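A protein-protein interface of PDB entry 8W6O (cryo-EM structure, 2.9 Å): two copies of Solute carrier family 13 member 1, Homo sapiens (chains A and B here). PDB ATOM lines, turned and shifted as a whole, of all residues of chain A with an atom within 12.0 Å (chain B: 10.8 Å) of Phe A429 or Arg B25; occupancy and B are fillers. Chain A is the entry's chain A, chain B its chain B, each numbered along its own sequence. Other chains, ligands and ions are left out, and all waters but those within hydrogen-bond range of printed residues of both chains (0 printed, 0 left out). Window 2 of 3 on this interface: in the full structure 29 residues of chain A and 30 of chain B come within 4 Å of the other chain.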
ATOM      1  N   PHE A 410       1.639 -19.727  11.911  1.00  0.00           N
ATOM      2  CA  PHE A 410       2.448 -20.760  12.543  1.00  0.00           C
ATOM      3  C   PHE A 410       1.621 -21.788  13.300  1.00  0.00           C
ATOM      4  O   PHE A 410       2.149 -22.848  13.645  1.00  0.00           O
ATOM      5  CB  PHE A 410       3.446 -20.132  13.514  1.00  0.00           C
ATOM      6  CG  PHE A 410       4.382 -19.146  12.884  1.00  0.00           C
ATOM      7  CD1 PHE A 410       5.502 -19.577  12.197  1.00  0.00           C
ATOM      8  CD2 PHE A 410       4.159 -17.786  13.007  1.00  0.00           C
ATOM      9  CE1 PHE A 410       6.375 -18.671  11.631  1.00  0.00           C
ATOM     10  CE2 PHE A 410       5.029 -16.874  12.442  1.00  0.00           C
ATOM     11  CZ  PHE A 410       6.138 -17.321  11.753  1.00  0.00           C
ATOM     12  N   LEU A 411       0.352 -21.504  13.575  1.00  0.00           N
ATOM     13  CA  LEU A 411      -0.485 -22.346  14.417  1.00  0.00           C
ATOM     14  C   LEU A 411      -1.506 -23.164  13.645  1.00  0.00           C
ATOM     15  O   LEU A 411      -1.720 -24.332  13.976  1.00  0.00           O
ATOM     16  CB  LEU A 411      -1.208 -21.481  15.458  1.00  0.00           C
ATOM     17  CG  LEU A 411      -2.316 -22.104  16.311  1.00  0.00           C
ATOM     18  CD1 LEU A 411      -1.759 -23.177  17.230  1.00  0.00           C
ATOM     19  CD2 LEU A 411      -3.043 -21.036  17.104  1.00  0.00           C
ATOM     20  N   ILE A 412      -2.125 -22.585  12.619  1.00  0.00           N
ATOM     21  CA  ILE A 412      -3.272 -23.205  11.941  1.00  0.00           C
ATOM     22  C   ILE A 412      -2.805 -24.431  11.163  1.00  0.00           C
ATOM     23  O   ILE A 412      -1.828 -24.344  10.399  1.00  0.00           O
ATOM     24  CB  ILE A 412      -3.962 -22.189  11.022  1.00  0.00           C
ATOM     25  CG1 ILE A 412      -4.810 -21.223  11.848  1.00  0.00           C
ATOM     26  CG2 ILE A 412      -4.847 -22.879   9.990  1.00  0.00           C
ATOM     27  CD1 ILE A 412      -5.457 -20.133  11.032  1.00  0.00           C
ATOM     28  N   PRO A 413      -3.442 -25.595  11.349  1.00  0.00           N
ATOM     29  CA  PRO A 413      -3.006 -26.809  10.649  1.00  0.00           C
ATOM     30  C   PRO A 413      -3.313 -26.801   9.160  1.00  0.00           C
ATOM     31  O   PRO A 413      -4.479 -26.791   8.755  1.00  0.00           O
ATOM     32  CB  PRO A 413      -3.786 -27.920  11.366  1.00  0.00           C
ATOM     33  CG  PRO A 413      -4.960 -27.246  11.971  1.00  0.00           C
ATOM     34  CD  PRO A 413      -4.530 -25.859  12.307  1.00  0.00           C
ATOM     35  N   ALA A 414      -2.272 -26.801   8.334  1.00  0.00           N
ATOM     36  CA  ALA A 414      -2.453 -27.080   6.919  1.00  0.00           C
ATOM     37  C   ALA A 414      -2.803 -28.551   6.734  1.00  0.00           C
ATOM     38  O   ALA A 414      -2.523 -29.389   7.596  1.00  0.00           O
ATOM     39  CB  ALA A 414      -1.185 -26.739   6.136  1.00  0.00           C
ATOM     40  N   LYS A 415      -3.407 -28.878   5.592  1.00  0.00           N
ATOM     41  CA  LYS A 415      -3.755 -30.274   5.344  1.00  0.00           C
ATOM     42  C   LYS A 415      -2.593 -31.048   4.731  1.00  0.00           C
ATOM     43  O   LYS A 415      -2.756 -31.720   3.707  1.00  0.00           O
ATOM     44  CB  LYS A 415      -4.992 -30.383   4.447  1.00  0.00           C
ATOM     45  CG  LYS A 415      -6.307 -29.958   5.098  1.00  0.00           C
ATOM     46  CD  LYS A 415      -6.756 -30.905   6.208  1.00  0.00           C
ATOM     47  CE  LYS A 415      -6.654 -30.261   7.585  1.00  0.00           C
ATOM     48  NZ  LYS A 415      -7.219 -31.133   8.646  1.00  0.00           N
ATOM     49  N   THR A 416      -1.423 -30.963   5.358  1.00  0.00           N
ATOM     50  CA  THR A 416      -0.252 -31.769   5.036  1.00  0.00           C
ATOM     51  C   THR A 416       0.127 -32.468   6.335  1.00  0.00           C
ATOM     52  O   THR A 416       0.892 -31.930   7.140  1.00  0.00           O
ATOM     53  CB  THR A 416       0.900 -30.926   4.491  1.00  0.00           C
ATOM     54  OG1 THR A 416       1.282 -29.952   5.470  1.00  0.00           O
ATOM     55  CG2 THR A 416       0.499 -30.227   3.197  1.00  0.00           C
ATOM     56  N   LEU A 417      -0.429 -33.658   6.546  1.00  0.00           N
ATOM     57  CA  LEU A 417      -0.144 -34.426   7.750  1.00  0.00           C
ATOM     58  C   LEU A 417       1.258 -35.008   7.663  1.00  0.00           C
ATOM     59  O   LEU A 417       1.549 -35.814   6.774  1.00  0.00           O
ATOM     60  CB  LEU A 417      -1.175 -35.535   7.925  1.00  0.00           C
ATOM     61  CG  LEU A 417      -2.369 -35.246   8.834  1.00  0.00           C
ATOM     62  CD1 LEU A 417      -3.360 -34.309   8.160  1.00  0.00           C
ATOM     63  CD2 LEU A 417      -3.046 -36.547   9.231  1.00  0.00           C
ATOM     64  N   THR A 418       2.128 -34.596   8.577  1.00  0.00           N
ATOM     65  CA  THR A 418       3.487 -35.111   8.613  1.00  0.00           C
ATOM     66  C   THR A 418       3.507 -36.479   9.281  1.00  0.00           C
ATOM     67  O   THR A 418       2.968 -37.449   8.749  1.00  0.00           O
ATOM     68  CB  THR A 418       4.439 -34.153   9.359  1.00  0.00           C
ATOM     69  OG1 THR A 418       4.705 -33.009   8.537  1.00  0.00           O
ATOM     70  CG2 THR A 418       5.753 -34.841   9.683  1.00  0.00           C
ATOM     71  N   PHE A 429       0.945 -39.055  11.780  1.00  0.00           N
ATOM     72  CA  PHE A 429       1.323 -39.025  13.188  1.00  0.00           C
ATOM     73  C   PHE A 429       1.512 -37.599  13.691  1.00  0.00           C
ATOM     74  O   PHE A 429       1.783 -37.386  14.872  1.00  0.00           O
ATOM     75  CB  PHE A 429       2.604 -39.838  13.414  1.00  0.00           C
ATOM     76  CG  PHE A 429       3.877 -39.086  13.109  1.00  0.00           C
ATOM     77  CD1 PHE A 429       4.278 -38.876  11.797  1.00  0.00           C
ATOM     78  CD2 PHE A 429       4.691 -38.621  14.135  1.00  0.00           C
ATOM     79  CE1 PHE A 429       5.453 -38.197  11.516  1.00  0.00           C
ATOM     80  CE2 PHE A 429       5.863 -37.937  13.857  1.00  0.00           C
ATOM     81  CZ  PHE A 429       6.243 -37.727  12.547  1.00  0.00           C
ATOM     82  N   ASP A 430       1.370 -36.626  12.797  1.00  0.00           N
ATOM     83  CA  ASP A 430       1.662 -35.235  13.117  1.00  0.00           C
ATOM     84  C   ASP A 430       0.850 -34.343  12.186  1.00  0.00           C
ATOM     85  O   ASP A 430      -0.079 -34.798  11.512  1.00  0.00           O
ATOM     86  CB  ASP A 430       3.169 -34.969  13.001  1.00  0.00           C
ATOM     87  CG  ASP A 430       3.652 -33.901  13.962  1.00  0.00           C
ATOM     88  OD1 ASP A 430       2.812 -33.341  14.695  1.00  0.00           O
ATOM     89  OD2 ASP A 430       4.867 -33.614  13.977  1.00  0.00           O
ATOM     90  N   TYR A 431       1.193 -33.059  12.169  1.00  0.00           N
ATOM     91  CA  TYR A 431       0.667 -32.119  11.194  1.00  0.00           C
ATOM     92  C   TYR A 431       1.723 -31.051  10.962  1.00  0.00           C
ATOM     93  O   TYR A 431       2.712 -30.955  11.690  1.00  0.00           O
ATOM     94  CB  TYR A 431      -0.682 -31.522  11.639  1.00  0.00           C
ATOM     95  CG  TYR A 431      -0.640 -30.420  12.690  1.00  0.00           C
ATOM     96  CD1 TYR A 431      -0.563 -29.077  12.324  1.00  0.00           C
ATOM     97  CD2 TYR A 431      -0.723 -30.721  14.043  1.00  0.00           C
ATOM     98  CE1 TYR A 431      -0.536 -28.077  13.272  1.00  0.00           C
ATOM     99  CE2 TYR A 431      -0.701 -29.723  14.998  1.00  0.00           C
ATOM    100  CZ  TYR A 431      -0.609 -28.405  14.603  1.00  0.00           C
ATOM    101  OH  TYR A 431      -0.587 -27.400  15.540  1.00  0.00           O
ATOM    102  N   SER A 432       1.495 -30.244   9.931  1.00  0.00           N
ATOM    103  CA  SER A 432       2.395 -29.165   9.569  1.00  0.00           C
ATOM    104  C   SER A 432       1.593 -27.877   9.453  1.00  0.00           C
ATOM    105  O   SER A 432       0.449 -27.902   8.989  1.00  0.00           O
ATOM    106  CB  SER A 432       3.110 -29.476   8.246  1.00  0.00           C
ATOM    107  OG  SER A 432       4.035 -28.463   7.900  1.00  0.00           O
ATOM    108  N   PRO A 433       2.153 -26.740   9.874  1.00  0.00           N
ATOM    109  CA  PRO A 433       1.393 -25.484   9.814  1.00  0.00           C
ATOM    110  C   PRO A 433       1.347 -24.881   8.420  1.00  0.00           C
ATOM    111  O   PRO A 433       1.789 -25.505   7.450  1.00  0.00           O
ATOM    112  CB  PRO A 433       2.149 -24.578  10.790  1.00  0.00           C
ATOM    113  CG  PRO A 433       3.533 -25.082  10.761  1.00  0.00           C
ATOM    114  CD  PRO A 433       3.458 -26.561  10.531  1.00  0.00           C
ATOM    115  N   ARG B  24      -2.663 -38.139  19.568  1.00  0.00           N
ATOM    116  CA  ARG B  24      -3.296 -37.733  18.320  1.00  0.00           C
ATOM    117  C   ARG B  24      -2.290 -37.024  17.414  1.00  0.00           C
ATOM    118  O   ARG B  24      -1.090 -37.015  17.684  1.00  0.00           O
ATOM    119  CB  ARG B  24      -4.500 -36.828  18.596  1.00  0.00           C
ATOM    120  CG  ARG B  24      -5.720 -37.120  17.730  1.00  0.00           C
ATOM    121  CD  ARG B  24      -6.866 -36.175  18.039  1.00  0.00           C
ATOM    122  NE  ARG B  24      -7.572 -36.547  19.260  1.00  0.00           N
ATOM    123  CZ  ARG B  24      -7.423 -35.925  20.424  1.00  0.00           C
ATOM    124  NH1 ARG B  24      -6.587 -34.903  20.527  1.00  0.00           N
ATOM    125  NH2 ARG B  24      -8.107 -36.328  21.484  1.00  0.00           N
ATOM    126  N   ARG B  25      -2.795 -36.436  16.332  1.00  0.00           N
ATOM    127  CA  ARG B  25      -1.993 -35.736  15.338  1.00  0.00           C
ATOM    128  C   ARG B  25      -2.018 -34.233  15.565  1.00  0.00           C
ATOM    129  O   ARG B  25      -0.969 -33.584  15.591  1.00  0.00           O
ATOM    130  CB  ARG B  25      -2.502 -36.048  13.923  1.00  0.00           C
ATOM    131  CG  ARG B  25      -2.095 -37.398  13.344  1.00  0.00           C
ATOM    132  CD  ARG B  25      -3.022 -38.515  13.803  1.00  0.00           C
ATOM    133  NE  ARG B  25      -4.403 -38.283  13.392  1.00  0.00           N
ATOM    134  CZ  ARG B  25      -5.450 -38.927  13.900  1.00  0.00           C
ATOM    135  NH1 ARG B  25      -6.673 -38.653  13.466  1.00  0.00           N
ATOM    136  NH2 ARG B  25      -5.276 -39.840  14.846  1.00  0.00           N
ATOM    137  N   PHE B  26      -3.213 -33.675  15.741  1.00  0.00           N
ATOM    138  CA  PHE B  26      -3.396 -32.259  16.034  1.00  0.00           C
ATOM    139  C   PHE B  26      -3.309 -32.022  17.543  1.00  0.00           C
ATOM    140  O   PHE B  26      -4.258 -31.603  18.200  1.00  0.00           O
ATOM    141  CB  PHE B  26      -4.726 -31.779  15.469  1.00  0.00           C
ATOM    142  CG  PHE B  26      -4.935 -32.134  14.023  1.00  0.00           C
ATOM    143  CD1 PHE B  26      -4.083 -31.647  13.045  1.00  0.00           C
ATOM    144  CD2 PHE B  26      -5.986 -32.953  13.644  1.00  0.00           C
ATOM    145  CE1 PHE B  26      -4.277 -31.973  11.715  1.00  0.00           C
ATOM    146  CE2 PHE B  26      -6.183 -33.281  12.316  1.00  0.00           C
ATOM    147  CZ  PHE B  26      -5.327 -32.790  11.353  1.00  0.00           C
ATOM    148  N   LEU B  27      -2.128 -32.312  18.088  1.00  0.00           N
ATOM    149  CA  LEU B  27      -1.927 -32.272  19.532  1.00  0.00           C
ATOM    150  C   LEU B  27      -1.684 -30.853  20.022  1.00  0.00           C
ATOM    151  O   LEU B  27      -2.369 -30.372  20.930  1.00  0.00           O
ATOM    152  CB  LEU B  27      -0.753 -33.170  19.925  1.00  0.00           C
ATOM    153  CG  LEU B  27      -1.024 -34.665  20.047  1.00  0.00           C
ATOM    154  CD1 LEU B  27       0.206 -35.375  20.581  1.00  0.00           C
ATOM    155  CD2 LEU B  27      -2.227 -34.911  20.937  1.00  0.00           C
ATOM    156  N   PHE B  28      -0.699 -30.169  19.446  1.00  0.00           N
ATOM    157  CA  PHE B  28      -0.332 -28.851  19.932  1.00  0.00           C
ATOM    158  C   PHE B  28      -1.028 -27.726  19.180  1.00  0.00           C
ATOM    159  O   PHE B  28      -0.511 -26.604  19.149  1.00  0.00           O
ATOM    160  CB  PHE B  28       1.192 -28.660  19.915  1.00  0.00           C
ATOM    161  CG  PHE B  28       1.866 -29.022  18.616  1.00  0.00           C
ATOM    162  CD1 PHE B  28       2.340 -30.307  18.394  1.00  0.00           C
ATOM    163  CD2 PHE B  28       2.086 -28.059  17.645  1.00  0.00           C
ATOM    164  CE1 PHE B  28       2.980 -30.634  17.211  1.00  0.00           C
ATOM    165  CE2 PHE B  28       2.728 -28.379  16.460  1.00  0.00           C
ATOM    166  CZ  PHE B  28       3.174 -29.667  16.245  1.00  0.00           C
ATOM    167  N   VAL B  29      -2.187 -27.994  18.580  1.00  0.00           N
ATOM    168  CA  VAL B  29      -3.110 -26.914  18.251  1.00  0.00           C
ATOM    169  C   VAL B  29      -4.174 -26.877  19.344  1.00  0.00           C
ATOM    170  O   VAL B  29      -4.521 -25.799  19.835  1.00  0.00           O
ATOM    171  CB  VAL B  29      -3.687 -27.030  16.815  1.00  0.00           C
ATOM    172  CG1 VAL B  29      -4.566 -28.256  16.591  1.00  0.00           C
ATOM    173  CG2 VAL B  29      -4.465 -25.767  16.446  1.00  0.00           C
ATOM    174  N   VAL B  30      -4.623 -28.040  19.814  1.00  0.00           N
ATOM    175  CA  VAL B  30      -5.610 -28.044  20.881  1.00  0.00           C
ATOM    176  C   VAL B  30      -4.950 -27.837  22.240  1.00  0.00           C
ATOM    177  O   VAL B  30      -5.568 -27.261  23.133  1.00  0.00           O
ATOM    178  CB  VAL B  30      -6.476 -29.319  20.861  1.00  0.00           C
ATOM    179  CG1 VAL B  30      -7.283 -29.390  19.575  1.00  0.00           C
ATOM    180  CG2 VAL B  30      -5.644 -30.572  21.033  1.00  0.00           C
ATOM    181  N   PHE B  31      -3.683 -28.233  22.402  1.00  0.00           N
ATOM    182  CA  PHE B  31      -2.963 -27.879  23.620  1.00  0.00           C
ATOM    183  C   PHE B  31      -2.667 -26.387  23.674  1.00  0.00           C
ATOM    184  O   PHE B  31      -2.623 -25.810  24.761  1.00  0.00           O
ATOM    185  CB  PHE B  31      -1.667 -28.682  23.737  1.00  0.00           C
ATOM    186  CG  PHE B  31      -0.840 -28.332  24.948  1.00  0.00           C
ATOM    187  CD1 PHE B  31      -1.204 -28.789  26.205  1.00  0.00           C
ATOM    188  CD2 PHE B  31       0.301 -27.550  24.829  1.00  0.00           C
ATOM    189  CE1 PHE B  31      -0.450 -28.469  27.320  1.00  0.00           C
ATOM    190  CE2 PHE B  31       1.055 -27.225  25.942  1.00  0.00           C
ATOM    191  CZ  PHE B  31       0.678 -27.688  27.187  1.00  0.00           C
ATOM    192  N   THR B  32      -2.467 -25.748  22.523  1.00  0.00           N
ATOM    193  CA  THR B  32      -2.278 -24.302  22.515  1.00  0.00           C
ATOM    194  C   THR B  32      -3.584 -23.580  22.822  1.00  0.00           C
ATOM    195  O   THR B  32      -3.631 -22.711  23.699  1.00  0.00           O
ATOM    196  CB  THR B  32      -1.699 -23.854  21.171  1.00  0.00           C
ATOM    197  OG1 THR B  32      -0.314 -24.210  21.108  1.00  0.00           O
ATOM    198  CG2 THR B  32      -1.825 -22.347  20.993  1.00  0.00           C
ATOM    199  N   ALA B  65       5.178 -26.147  22.026  1.00  0.00           N
ATOM    200  CA  ALA B  65       3.992 -26.158  21.180  1.00  0.00           C
ATOM    201  C   ALA B  65       4.124 -25.179  20.024  1.00  0.00           C
ATOM    202  O   ALA B  65       3.575 -25.419  18.945  1.00  0.00           O
ATOM    203  CB  ALA B  65       2.751 -25.836  22.009  1.00  0.00           C
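OH of Tyr A431 lies close to N of Val B29, at 3.5 Å.
The backbone carbonyl oxygen (O) of Phe B28 is in hydrogen-bond range of the side-chain hydroxyl (OG1) of Thr B32 (3.1 Å).
Among the printed residues, merely in contact across the chains: Leu A411 with Val B29 (3.8 Å), Leu A411 with Thr B32 (3.9 Å), Lys A415 with Phe B26 (3.7 Å), Phe A429 with Arg B25 (3.6 Å), Asp A430 with Arg B25 (3.6 Å), Asp A430 with Phe B28 (3.7 Å), Tyr A431 with Arg B25 (3.3 Å), Tyr A431 with Phe B26 (3.6 Å) and Tyr A431 with Phe B28 (3.5 Å).
Arg B25 touches just these residues of chain A: Phe A429 (3.6 Å), Asp A430 (3.6 Å) and Tyr A431 (3.3 Å). No residue of chain B comes within 4 Å of Thr A418. Tyr A431 touches just these residues of chain B: Arg B25, Phe B26, Phe B28 and Val B29. No residue of chain A comes within 4 Å of Arg B24. Of chain A, only Lys A415 and Tyr A431 come within 4 Å of Phe B26. Phe B28 touches just these residues of chain A: Asp A430 (3.7 Å) and Tyr A431 (3.5 Å). Printed residues of chain A within 4 Å of Val B29: Leu A411 (3.8 Å) and Tyr A431 (3.4 Å). Of the printed residues of chain A, Thr B32 touches Leu A411 (3.9 Å). Of the printed residues of chain B, Leu A411 touches Val B29 and Thr B32. The nearest residue of chain B that does not touch Phe A429 is Arg B24 (4.04 Å).
Hydrophobic or aromatic side chains of chain B within 4 Å of the printed part of chain A: Phe B26, Phe B28 and Val B29. Hydrophobic or aromatic side chains of chain A within 4 Å of the printed part of chain B: Leu A411 and Tyr A431. Among the printed residues, 10 pairs touch across the chains. Among the printed residues, no Asp or Glu carboxylate lies within 4 Å of a Lys or Arg side-chain nitrogen of the other chain.
No position is printed for both chains.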
